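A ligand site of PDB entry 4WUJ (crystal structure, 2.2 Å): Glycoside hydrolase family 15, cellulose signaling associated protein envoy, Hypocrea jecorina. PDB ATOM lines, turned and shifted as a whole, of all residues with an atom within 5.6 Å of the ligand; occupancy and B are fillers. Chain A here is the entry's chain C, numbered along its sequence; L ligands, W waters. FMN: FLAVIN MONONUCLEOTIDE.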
ATOM      1  N   THR A  41      24.642   3.284  21.133  1.00  0.00           N
ATOM      2  CA  THR A  41      25.872   4.006  20.868  1.00  0.00           C
ATOM      3  C   THR A  41      25.525   5.457  20.539  1.00  0.00           C
ATOM      4  O   THR A  41      24.442   5.767  20.025  1.00  0.00           O
ATOM      5  CB  THR A  41      26.739   3.377  19.728  1.00  0.00           C
ATOM      6  OG1 THR A  41      26.055   3.497  18.465  1.00  0.00           O
ATOM      7  CG2 THR A  41      27.013   1.923  19.998  1.00  0.00           C
ATOM      8  N   LEU A  42      26.431   6.325  20.901  1.00  0.00           N
ATOM      9  CA  LEU A  42      26.348   7.724  20.575  1.00  0.00           C
ATOM     10  C   LEU A  42      27.649   8.045  19.824  1.00  0.00           C
ATOM     11  O   LEU A  42      28.763   7.753  20.303  1.00  0.00           O
ATOM     12  CB  LEU A  42      26.260   8.539  21.867  1.00  0.00           C
ATOM     13  CG  LEU A  42      25.907  10.010  21.824  1.00  0.00           C
ATOM     14  CD1 LEU A  42      24.631  10.338  21.056  1.00  0.00           C
ATOM     15  CD2 LEU A  42      25.771  10.419  23.283  1.00  0.00           C
ATOM     16  N   CYS A  43      27.488   8.638  18.642  1.00  0.00           N
ATOM     17  CA  CYS A  43      28.632   8.933  17.777  1.00  0.00           C
ATOM     18  C   CYS A  43      28.636  10.409  17.445  1.00  0.00           C
ATOM     19  O   CYS A  43      27.584  10.985  17.195  1.00  0.00           O
ATOM     20  CB  CYS A  43      28.569   8.112  16.505  1.00  0.00           C
ATOM     21  SG  CYS A  43      28.763   6.322  16.772  1.00  0.00           S
ATOM     22  N   ILE A  45      29.223  12.667  14.791  1.00  0.00           N
ATOM     23  CA  ILE A  45      29.482  12.639  13.353  1.00  0.00           C
ATOM     24  C   ILE A  45      30.159  13.934  12.764  1.00  0.00           C
ATOM     25  O   ILE A  45      30.518  13.959  11.593  1.00  0.00           O
ATOM     26  CB  ILE A  45      28.207  12.279  12.594  1.00  0.00           C
ATOM     27  CG1 ILE A  45      27.184  13.385  12.737  1.00  0.00           C
ATOM     28  CG2 ILE A  45      27.608  10.906  13.107  1.00  0.00           C
ATOM     29  CD1 ILE A  45      26.236  13.426  11.580  1.00  0.00           C
ATOM     30  N   ASP A  49      35.451  10.342  10.986  1.00  0.00           N
ATOM     31  CA  ASP A  49      34.968   8.961  10.942  1.00  0.00           C
ATOM     32  C   ASP A  49      33.986   8.583  12.077  1.00  0.00           C
ATOM     33  O   ASP A  49      33.984   7.445  12.550  1.00  0.00           O
ATOM     34  CB  ASP A  49      36.157   7.974  10.913  1.00  0.00           C
ATOM     35  CG  ASP A  49      35.813   6.669  10.249  1.00  0.00           C
ATOM     36  OD1 ASP A  49      34.904   6.645   9.381  1.00  0.00           O
ATOM     37  OD2 ASP A  49      36.438   5.640  10.594  1.00  0.00           O
ATOM     38  N   ALA A  50      33.181   9.552  12.517  1.00  0.00           N
ATOM     39  CA  ALA A  50      32.036   9.316  13.394  1.00  0.00           C
ATOM     40  C   ALA A  50      32.334   8.443  14.608  1.00  0.00           C
ATOM     41  O   ALA A  50      31.676   7.410  14.798  1.00  0.00           O
ATOM     42  CB  ALA A  50      30.870   8.665  12.548  1.00  0.00           C
ATOM     43  N   PHE A  59      25.221  -2.352  25.207  1.00  0.00           N
ATOM     44  CA  PHE A  59      26.046  -2.554  24.005  1.00  0.00           C
ATOM     45  C   PHE A  59      27.194  -3.497  24.309  1.00  0.00           C
ATOM     46  O   PHE A  59      27.493  -4.385  23.523  1.00  0.00           O
ATOM     47  CB  PHE A  59      26.587  -1.245  23.455  1.00  0.00           C
ATOM     48  CG  PHE A  59      27.542  -1.396  22.262  1.00  0.00           C
ATOM     49  CD1 PHE A  59      27.046  -1.406  20.929  1.00  0.00           C
ATOM     50  CD2 PHE A  59      28.931  -1.514  22.470  1.00  0.00           C
ATOM     51  CE1 PHE A  59      27.918  -1.518  19.827  1.00  0.00           C
ATOM     52  CE2 PHE A  59      29.822  -1.631  21.388  1.00  0.00           C
ATOM     53  CZ  PHE A  59      29.316  -1.609  20.051  1.00  0.00           C
ATOM     54  N   ASN A  74      34.784   3.937  14.840  1.00  0.00           N
ATOM     55  CA  ASN A  74      33.571   3.901  14.012  1.00  0.00           C
ATOM     56  C   ASN A  74      32.883   2.579  14.250  1.00  0.00           C
ATOM     57  O   ASN A  74      33.544   1.562  14.487  1.00  0.00           O
ATOM     58  CB  ASN A  74      33.887   4.034  12.525  1.00  0.00           C
ATOM     59  CG  ASN A  74      32.653   4.150  11.669  1.00  0.00           C
ATOM     60  OD1 ASN A  74      31.990   3.172  11.403  1.00  0.00           O
ATOM     61  ND2 ASN A  74      32.339   5.372  11.227  1.00  0.00           N
ATOM     62  N   CYS A  75      31.560   2.617  14.207  1.00  0.00           N
ATOM     63  CA  CYS A  75      30.717   1.437  14.457  1.00  0.00           C
ATOM     64  C   CYS A  75      30.840   0.288  13.443  1.00  0.00           C
ATOM     65  O   CYS A  75      30.321  -0.832  13.702  1.00  0.00           O
ATOM     66  CB  CYS A  75      29.284   1.883  14.524  1.00  0.00           C
ATOM     67  SG  CYS A  75      28.875   2.650  16.134  1.00  0.00           S
ATOM     68  N   ARG A  76      31.514   0.515  12.315  1.00  0.00           N
ATOM     69  CA  ARG A  76      31.504  -0.484  11.238  1.00  0.00           C
ATOM     70  C   ARG A  76      32.311  -1.744  11.642  1.00  0.00           C
ATOM     71  O   ARG A  76      32.175  -2.790  11.025  1.00  0.00           O
ATOM     72  CB  ARG A  76      32.039   0.086   9.889  1.00  0.00           C
ATOM     73  CG  ARG A  76      33.547   0.311   9.970  1.00  0.00           C
ATOM     74  CD  ARG A  76      34.172   0.740   8.618  1.00  0.00           C
ATOM     75  NE  ARG A  76      33.596   2.008   8.190  1.00  0.00           N
ATOM     76  CZ  ARG A  76      34.071   3.198   8.521  1.00  0.00           C
ATOM     77  NH1 ARG A  76      35.104   3.293   9.350  1.00  0.00           N
ATOM     78  NH2 ARG A  76      33.473   4.288   8.078  1.00  0.00           N
ATOM     79  N   LEU A  78      31.657  -3.643  13.629  1.00  0.00           N
ATOM     80  CA  LEU A  78      30.658  -4.641  13.979  1.00  0.00           C
ATOM     81  C   LEU A  78      30.295  -5.509  12.793  1.00  0.00           C
ATOM     82  O   LEU A  78      29.704  -6.583  12.924  1.00  0.00           O
ATOM     83  CB  LEU A  78      29.401  -3.961  14.528  1.00  0.00           C
ATOM     84  CG  LEU A  78      29.504  -3.303  15.916  1.00  0.00           C
ATOM     85  CD1 LEU A  78      28.245  -2.506  16.193  1.00  0.00           C
ATOM     86  CD2 LEU A  78      29.695  -4.365  16.980  1.00  0.00           C
ATOM     87  N   GLN A  79      30.612  -5.028  11.602  1.00  0.00           N
ATOM     88  CA  GLN A  79      30.344  -5.803  10.397  1.00  0.00           C
ATOM     89  C   GLN A  79      31.461  -6.820  10.138  1.00  0.00           C
ATOM     90  O   GLN A  79      31.365  -7.610   9.218  1.00  0.00           O
ATOM     91  CB  GLN A  79      30.178  -4.874   9.199  1.00  0.00           C
ATOM     92  CG  GLN A  79      28.923  -4.079   9.202  1.00  0.00           C
ATOM     93  CD  GLN A  79      29.110  -2.722   8.510  1.00  0.00           C
ATOM     94  OE1 GLN A  79      29.907  -2.593   7.589  1.00  0.00           O
ATOM     95  NE2 GLN A  79      28.361  -1.711   8.965  1.00  0.00           N
ATOM     96  N   VAL A  94      24.418  -1.436   4.753  1.00  0.00           N
ATOM     97  CA  VAL A  94      25.548  -0.530   4.864  1.00  0.00           C
ATOM     98  C   VAL A  94      25.357   0.802   4.121  1.00  0.00           C
ATOM     99  O   VAL A  94      25.529   1.871   4.749  1.00  0.00           O
ATOM    100  CB  VAL A  94      26.862  -1.223   4.414  1.00  0.00           C
ATOM    101  CG1 VAL A  94      28.032  -0.247   4.416  1.00  0.00           C
ATOM    102  CG2 VAL A  94      27.151  -2.378   5.342  1.00  0.00           C
ATOM    103  N   GLN A  95      24.978   0.775   2.833  1.00  0.00           N
ATOM    104  CA  GLN A  95      24.763   2.019   2.058  1.00  0.00           C
ATOM    105  C   GLN A  95      23.597   2.834   2.600  1.00  0.00           C
ATOM    106  O   GLN A  95      23.640   4.078   2.638  1.00  0.00           O
ATOM    107  CB  GLN A  95      24.372   1.808   0.582  1.00  0.00           C
ATOM    108  CG  GLN A  95      25.009   0.712  -0.201  1.00  0.00           C
ATOM    109  CD  GLN A  95      24.463   0.702  -1.653  1.00  0.00           C
ATOM    110  OE1 GLN A  95      24.446   1.735  -2.350  1.00  0.00           O
ATOM    111  NE2 GLN A  95      23.975  -0.477  -2.085  1.00  0.00           N
ATOM    112  N   MET A  97      22.512   2.869   5.626  1.00  0.00           N
ATOM    113  CA  MET A  97      22.970   3.541   6.842  1.00  0.00           C
ATOM    114  C   MET A  97      23.852   4.751   6.447  1.00  0.00           C
ATOM    115  O   MET A  97      23.647   5.867   6.904  1.00  0.00           O
ATOM    116  CB  MET A  97      23.733   2.582   7.738  1.00  0.00           C
ATOM    117  CG  MET A  97      22.817   1.660   8.555  1.00  0.00           C
ATOM    118  SD  MET A  97      23.672   0.601   9.743  1.00  0.00           S
ATOM    119  CE  MET A  97      24.771  -0.346   8.727  1.00  0.00           C
ATOM    120  N   ARG A  98      24.773   4.514   5.507  1.00  0.00           N
ATOM    121  CA  ARG A  98      25.728   5.528   5.077  1.00  0.00           C
ATOM    122  C   ARG A  98      25.027   6.769   4.573  1.00  0.00           C
ATOM    123  O   ARG A  98      25.410   7.912   4.930  1.00  0.00           O
ATOM    124  CB  ARG A  98      26.641   4.960   3.993  1.00  0.00           C
ATOM    125  CG  ARG A  98      27.704   5.940   3.583  1.00  0.00           C
ATOM    126  CD  ARG A  98      28.805   5.319   2.753  1.00  0.00           C
ATOM    127  NE  ARG A  98      28.279   4.783   1.509  1.00  0.00           N
ATOM    128  CZ  ARG A  98      28.265   3.497   1.177  1.00  0.00           C
ATOM    129  NH1 ARG A  98      28.797   2.573   1.970  1.00  0.00           N
ATOM    130  NH2 ARG A  98      27.734   3.138   0.019  1.00  0.00           N
ATOM    131  N   ILE A 101      22.834   8.522   7.302  1.00  0.00           N
ATOM    132  CA  ILE A 101      23.676   9.276   8.257  1.00  0.00           C
ATOM    133  C   ILE A 101      24.033  10.599   7.626  1.00  0.00           C
ATOM    134  O   ILE A 101      23.924  11.664   8.256  1.00  0.00           O
ATOM    135  CB  ILE A 101      24.960   8.494   8.596  1.00  0.00           C
ATOM    136  CG1 ILE A 101      24.635   7.353   9.569  1.00  0.00           C
ATOM    137  CG2 ILE A 101      26.006   9.438   9.183  1.00  0.00           C
ATOM    138  CD1 ILE A 101      25.730   6.335   9.704  1.00  0.00           C
ATOM    139  N   ILE A 111      20.861  -6.064   9.606  1.00  0.00           N
ATOM    140  CA  ILE A 111      22.133  -6.281   8.988  1.00  0.00           C
ATOM    141  C   ILE A 111      22.852  -7.284   9.828  1.00  0.00           C
ATOM    142  O   ILE A 111      22.592  -7.364  11.026  1.00  0.00           O
ATOM    143  CB  ILE A 111      22.975  -4.916   8.967  1.00  0.00           C
ATOM    144  CG1 ILE A 111      24.389  -5.146   8.469  1.00  0.00           C
ATOM    145  CG2 ILE A 111      23.017  -4.241  10.365  1.00  0.00           C
ATOM    146  CD1 ILE A 111      25.185  -3.835   8.324  1.00  0.00           C
ATOM    147  N   VAL A 112      23.813  -7.976   9.254  1.00  0.00           N
ATOM    148  CA  VAL A 112      24.586  -8.918  10.049  1.00  0.00           C
ATOM    149  C   VAL A 112      25.769  -8.267  10.677  1.00  0.00           C
ATOM    150  O   VAL A 112      26.616  -7.687   9.981  1.00  0.00           O
ATOM    151  CB  VAL A 112      25.054 -10.109   9.226  1.00  0.00           C
ATOM    152  CG1 VAL A 112      26.033 -10.969  10.043  1.00  0.00           C
ATOM    153  CG2 VAL A 112      23.818 -10.929   8.737  1.00  0.00           C
ATOM    154  N   ASN A 113      25.842  -8.338  12.000  1.00  0.00           N
ATOM    155  CA  ASN A 113      27.091  -8.036  12.694  1.00  0.00           C
ATOM    156  C   ASN A 113      27.677  -9.241  13.413  1.00  0.00           C
ATOM    157  O   ASN A 113      27.088 -10.326  13.464  1.00  0.00           O
ATOM    158  CB  ASN A 113      26.952  -6.866  13.688  1.00  0.00           C
ATOM    159  CG  ASN A 113      26.468  -5.589  13.035  1.00  0.00           C
ATOM    160  OD1 ASN A 113      25.830  -4.761  13.681  1.00  0.00           O
ATOM    161  ND2 ASN A 113      26.739  -5.438  11.727  1.00  0.00           N
ATOM    162  N   ASN A 123      21.311  -7.914  13.654  1.00  0.00           N
ATOM    163  CA  ASN A 123      21.189  -6.738  14.490  1.00  0.00           C
ATOM    164  C   ASN A 123      20.133  -5.832  13.905  1.00  0.00           C
ATOM    165  O   ASN A 123      20.216  -5.464  12.721  1.00  0.00           O
ATOM    166  CB  ASN A 123      22.564  -6.050  14.531  1.00  0.00           C
ATOM    167  CG  ASN A 123      22.593  -4.871  15.473  1.00  0.00           C
ATOM    168  OD1 ASN A 123      21.560  -4.464  16.008  1.00  0.00           O
ATOM    169  ND2 ASN A 123      23.790  -4.280  15.664  1.00  0.00           N
ATOM    170  N   VAL A 125      19.309  -2.365  13.759  1.00  0.00           N
ATOM    171  CA  VAL A 125      19.964  -1.098  14.040  1.00  0.00           C
ATOM    172  C   VAL A 125      19.099   0.015  13.601  1.00  0.00           C
ATOM    173  O   VAL A 125      18.611   0.048  12.462  1.00  0.00           O
ATOM    174  CB  VAL A 125      21.299  -0.972  13.278  1.00  0.00           C
ATOM    175  CG1 VAL A 125      21.939   0.333  13.590  1.00  0.00           C
ATOM    176  CG2 VAL A 125      22.247  -2.136  13.633  1.00  0.00           C
ATOM    177  N   ILE A 127      19.231   4.310  13.516  1.00  0.00           N
ATOM    178  CA  ILE A 127      20.086   5.451  13.708  1.00  0.00           C
ATOM    179  C   ILE A 127      19.258   6.699  13.617  1.00  0.00           C
ATOM    180  O   ILE A 127      18.522   6.912  12.659  1.00  0.00           O
ATOM    181  CB  ILE A 127      21.248   5.428  12.670  1.00  0.00           C
ATOM    182  CG1 ILE A 127      21.966   4.089  12.784  1.00  0.00           C
ATOM    183  CG2 ILE A 127      22.190   6.603  12.896  1.00  0.00           C
ATOM    184  CD1 ILE A 127      22.974   3.761  11.748  1.00  0.00           C
ATOM    185  N   ALA A 140      24.747  11.221  16.427  1.00  0.00           N
ATOM    186  CA  ALA A 140      23.867  10.201  15.955  1.00  0.00           C
ATOM    187  C   ALA A 140      23.757   9.222  17.084  1.00  0.00           C
ATOM    188  O   ALA A 140      24.760   8.902  17.744  1.00  0.00           O
ATOM    189  CB  ALA A 140      24.434   9.516  14.709  1.00  0.00           C
ATOM    190  N   VAL A 141      22.532   8.777  17.330  1.00  0.00           N
ATOM    191  CA  VAL A 141      22.240   7.753  18.316  1.00  0.00           C
ATOM    192  C   VAL A 141      21.868   6.520  17.566  1.00  0.00           C
ATOM    193  O   VAL A 141      20.959   6.554  16.748  1.00  0.00           O
ATOM    194  CB  VAL A 141      20.994   8.096  19.165  1.00  0.00           C
ATOM    195  CG1 VAL A 141      20.725   6.956  20.155  1.00  0.00           C
ATOM    196  CG2 VAL A 141      21.180   9.414  19.838  1.00  0.00           C
ATOM    197  N   GLY A 142      22.562   5.443  17.868  1.00  0.00           N
ATOM    198  CA  GLY A 142      22.205   4.138  17.370  1.00  0.00           C
ATOM    199  C   GLY A 142      21.686   3.222  18.466  1.00  0.00           C
ATOM    200  O   GLY A 142      22.191   3.204  19.602  1.00  0.00           O
ATOM    201  N   GLN A 144      20.953  -0.778  18.907  1.00  0.00           N
ATOM    202  CA  GLN A 144      21.133  -2.136  18.416  1.00  0.00           C
ATOM    203  C   GLN A 144      20.263  -3.137  19.243  1.00  0.00           C
ATOM    204  O   GLN A 144      19.902  -2.862  20.408  1.00  0.00           O
ATOM    205  CB  GLN A 144      22.578  -2.594  18.576  1.00  0.00           C
ATOM    206  CG  GLN A 144      23.641  -1.756  17.860  1.00  0.00           C
ATOM    207  CD  GLN A 144      24.046  -0.470  18.551  1.00  0.00           C
ATOM    208  OE1 GLN A 144      23.814  -0.250  19.781  1.00  0.00           O
ATOM    209  NE2 GLN A 144      24.652   0.418  17.766  1.00  0.00           N
HETATM  210  N1  FMN L   1      26.741  -0.464  11.659  1.00  0.00           N
HETATM  211  C2  FMN L   1      26.535  -1.778  12.032  1.00  0.00           C
HETATM  212  O2  FMN L   1      26.817  -2.692  11.256  1.00  0.00           O
HETATM  213  N3  FMN L   1      26.026  -2.075  13.295  1.00  0.00           N
HETATM  214  C4  FMN L   1      25.697  -1.083  14.186  1.00  0.00           C
HETATM  215  O4  FMN L   1      25.268  -1.387  15.289  1.00  0.00           O
HETATM  216  C4A FMN L   1      25.895   0.255  13.824  1.00  0.00           C
HETATM  217  N5  FMN L   1      25.594   1.283  14.707  1.00  0.00           N
HETATM  218  C5A FMN L   1      25.776   2.589  14.334  1.00  0.00           C
HETATM  219  C6  FMN L   1      25.449   3.575  15.241  1.00  0.00           C
HETATM  220  C7  FMN L   1      25.642   4.907  14.922  1.00  0.00           C
HETATM  221  C7M FMN L   1      25.259   5.943  15.927  1.00  0.00           C
HETATM  222  C8  FMN L   1      26.178   5.240  13.651  1.00  0.00           C
HETATM  223  C8M FMN L   1      26.393   6.693  13.297  1.00  0.00           C
HETATM  224  C9  FMN L   1      26.492   4.240  12.734  1.00  0.00           C
HETATM  225  C9A FMN L   1      26.302   2.901  13.068  1.00  0.00           C
HETATM  226  N10 FMN L   1      26.617   1.870  12.182  1.00  0.00           N
HETATM  227  C10 FMN L   1      26.418   0.550  12.558  1.00  0.00           C
HETATM  228  C1' FMN L   1      27.136   2.085  10.770  1.00  0.00           C
HETATM  229  C2' FMN L   1      28.609   2.322  10.558  1.00  0.00           C
HETATM  230  O2' FMN L   1      29.127   3.002  11.675  1.00  0.00           O
HETATM  231  C3' FMN L   1      28.780   3.076   9.206  1.00  0.00           C
HETATM  232  O3' FMN L   1      28.046   4.303   9.219  1.00  0.00           O
HETATM  233  C4' FMN L   1      28.300   2.213   8.021  1.00  0.00           C
HETATM  234  O4' FMN L   1      29.146   1.088   7.927  1.00  0.00           O
HETATM  235  C5' FMN L   1      28.219   2.980   6.686  1.00  0.00           C
HETATM  236  O5' FMN L   1      29.431   3.681   6.454  1.00  0.00           O
HETATM  237  P   FMN L   1      30.656   2.981   5.718  1.00  0.00           P
HETATM  238  O1P FMN L   1      31.784   4.000   5.756  1.00  0.00           O
HETATM  239  O2P FMN L   1      31.143   1.721   6.334  1.00  0.00           O
HETATM  240  O3P FMN L   1      30.273   2.709   4.291  1.00  0.00           O
HETATM  241  O   HOH W   1      29.324   6.099  11.011  1.00  0.00           O
HETATM  242  O   HOH W   2      29.954   5.363  13.894  1.00  0.00           O
HETATM  243  O   HOH W   3      34.440   3.115   4.785  1.00  0.00           O
HETATM  244  O   HOH W   4      28.645   6.672   7.594  1.00  0.00           O
HETATM  245  O   HOH W   5      31.285   6.369   6.154  1.00  0.00           O
HETATM  246  O   HOH W   6      31.534  -0.759   6.108  1.00  0.00           O
HETATM  247  O   HOH W   7      31.544   0.984   3.008  1.00  0.00           O
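An oxygen (O4) of the ligand is in hydrogen-bond range of the side-chain amide nitrogen of Asn 123, 3.3 Å away.
NH2 of Arg 76 is in salt-bridge range of O1P of the ligand, 2.9 Å away.
O2' of the ligand is in hydrogen-bond range of OD1 of Asn 74 (2.9 Å).
The side-chain amide oxygen (OD1) of Asn 113 lies within hydrogen-bond range of a nitrogen (N3) of the ligand, at 2.7 Å.
NE2 of Gln 144 sits close to O4 of the ligand.
The side-chain amide nitrogen (NE2) of Gln 79 sits at hydrogen-bond distance from an oxygen (O2) of the ligand, 2.9 Å away.
An oxygen (O3P) of the ligand lies within salt-bridge range of the guanidinium group of Arg 98 (2.8 Å).
NH1 of Arg 76 is in salt-bridge range of OD2 of Asp 49, 3.0 Å away.
The side-chain amide oxygen of Asn 74 lies within hydrogen-bond range of the backbone NH of Arg 76, 2.8 Å away.
The side-chain amide nitrogen (ND2) of Asn 123 sits at hydrogen-bond distance from the side-chain amide oxygen (OD1) of Asn 113 (2.9 Å).
The backbone carbonyl oxygen of Thr 41 lies within hydrogen-bond range of the backbone NH of Gly 142.
ND2 of Asn 74 is in hydrogen-bond range of O of Asp 49, at 3.0 Å.
SG of Cys 75 is in hydrogen-bond range of SG of Cys 43 (3.7 Å).
The backbone NH of Cys 43 is in hydrogen-bond range of the backbone carbonyl oxygen of Ala 140, 2.9 Å away.
The backbone carbonyl oxygen (O) of Ala 50 sits close to the side-chain sulfur (SG) of Cys 43, 3.7 Å away.
The side-chain sulfur of Met 97 lies close to a nitrogen (N1) of the ligand (3.8 Å).
Merely in contact with the ligand: Thr 41, Cys 43, Cys 75, Leu 78, Val 94, Ile 101, Ile 111, Val 125, Ile 127, Ala 140, Val 141 and Gly 142.
Hydrophobic or aromatic side chains within 4 Å of the ligand: Leu 78, Val 94, Met 97, Ile 101, Ile 111, Val 125, Ile 127 and Ala 140.
Within 4 Å of the ligand: Thr 41, Cys 43, Asn 74, Cys 75, Arg 76, Leu 78, Gln 79, Val 94, Met 97, Arg 98, Ile 101, Ile 111, Asn 113, Asn 123, Val 125, Ile 127, Ala 140, Val 141, Gly 142 and Gln 144.
The nearest printed residue that does not touch the ligand is Ile 45 (4.4 Å).
Water W7 bridges an oxygen (O3P) of the ligand and the guanidinium group (NH1) of Arg 98.
Water W6 lies within hydrogen-bond range of O2P of the ligand (2.5 Å) and OE1 of Gln 79 (2.9 Å).
Water W1 bridges O3' of the ligand and ND2 of Asn 74.
Water W2 lies within hydrogen-bond range of O of Ala 50 (2.8 Å), N of Cys 75 (3.2 Å), SG of Cys 43 (3.3 Å) and O2' of the ligand (3.3 Å).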
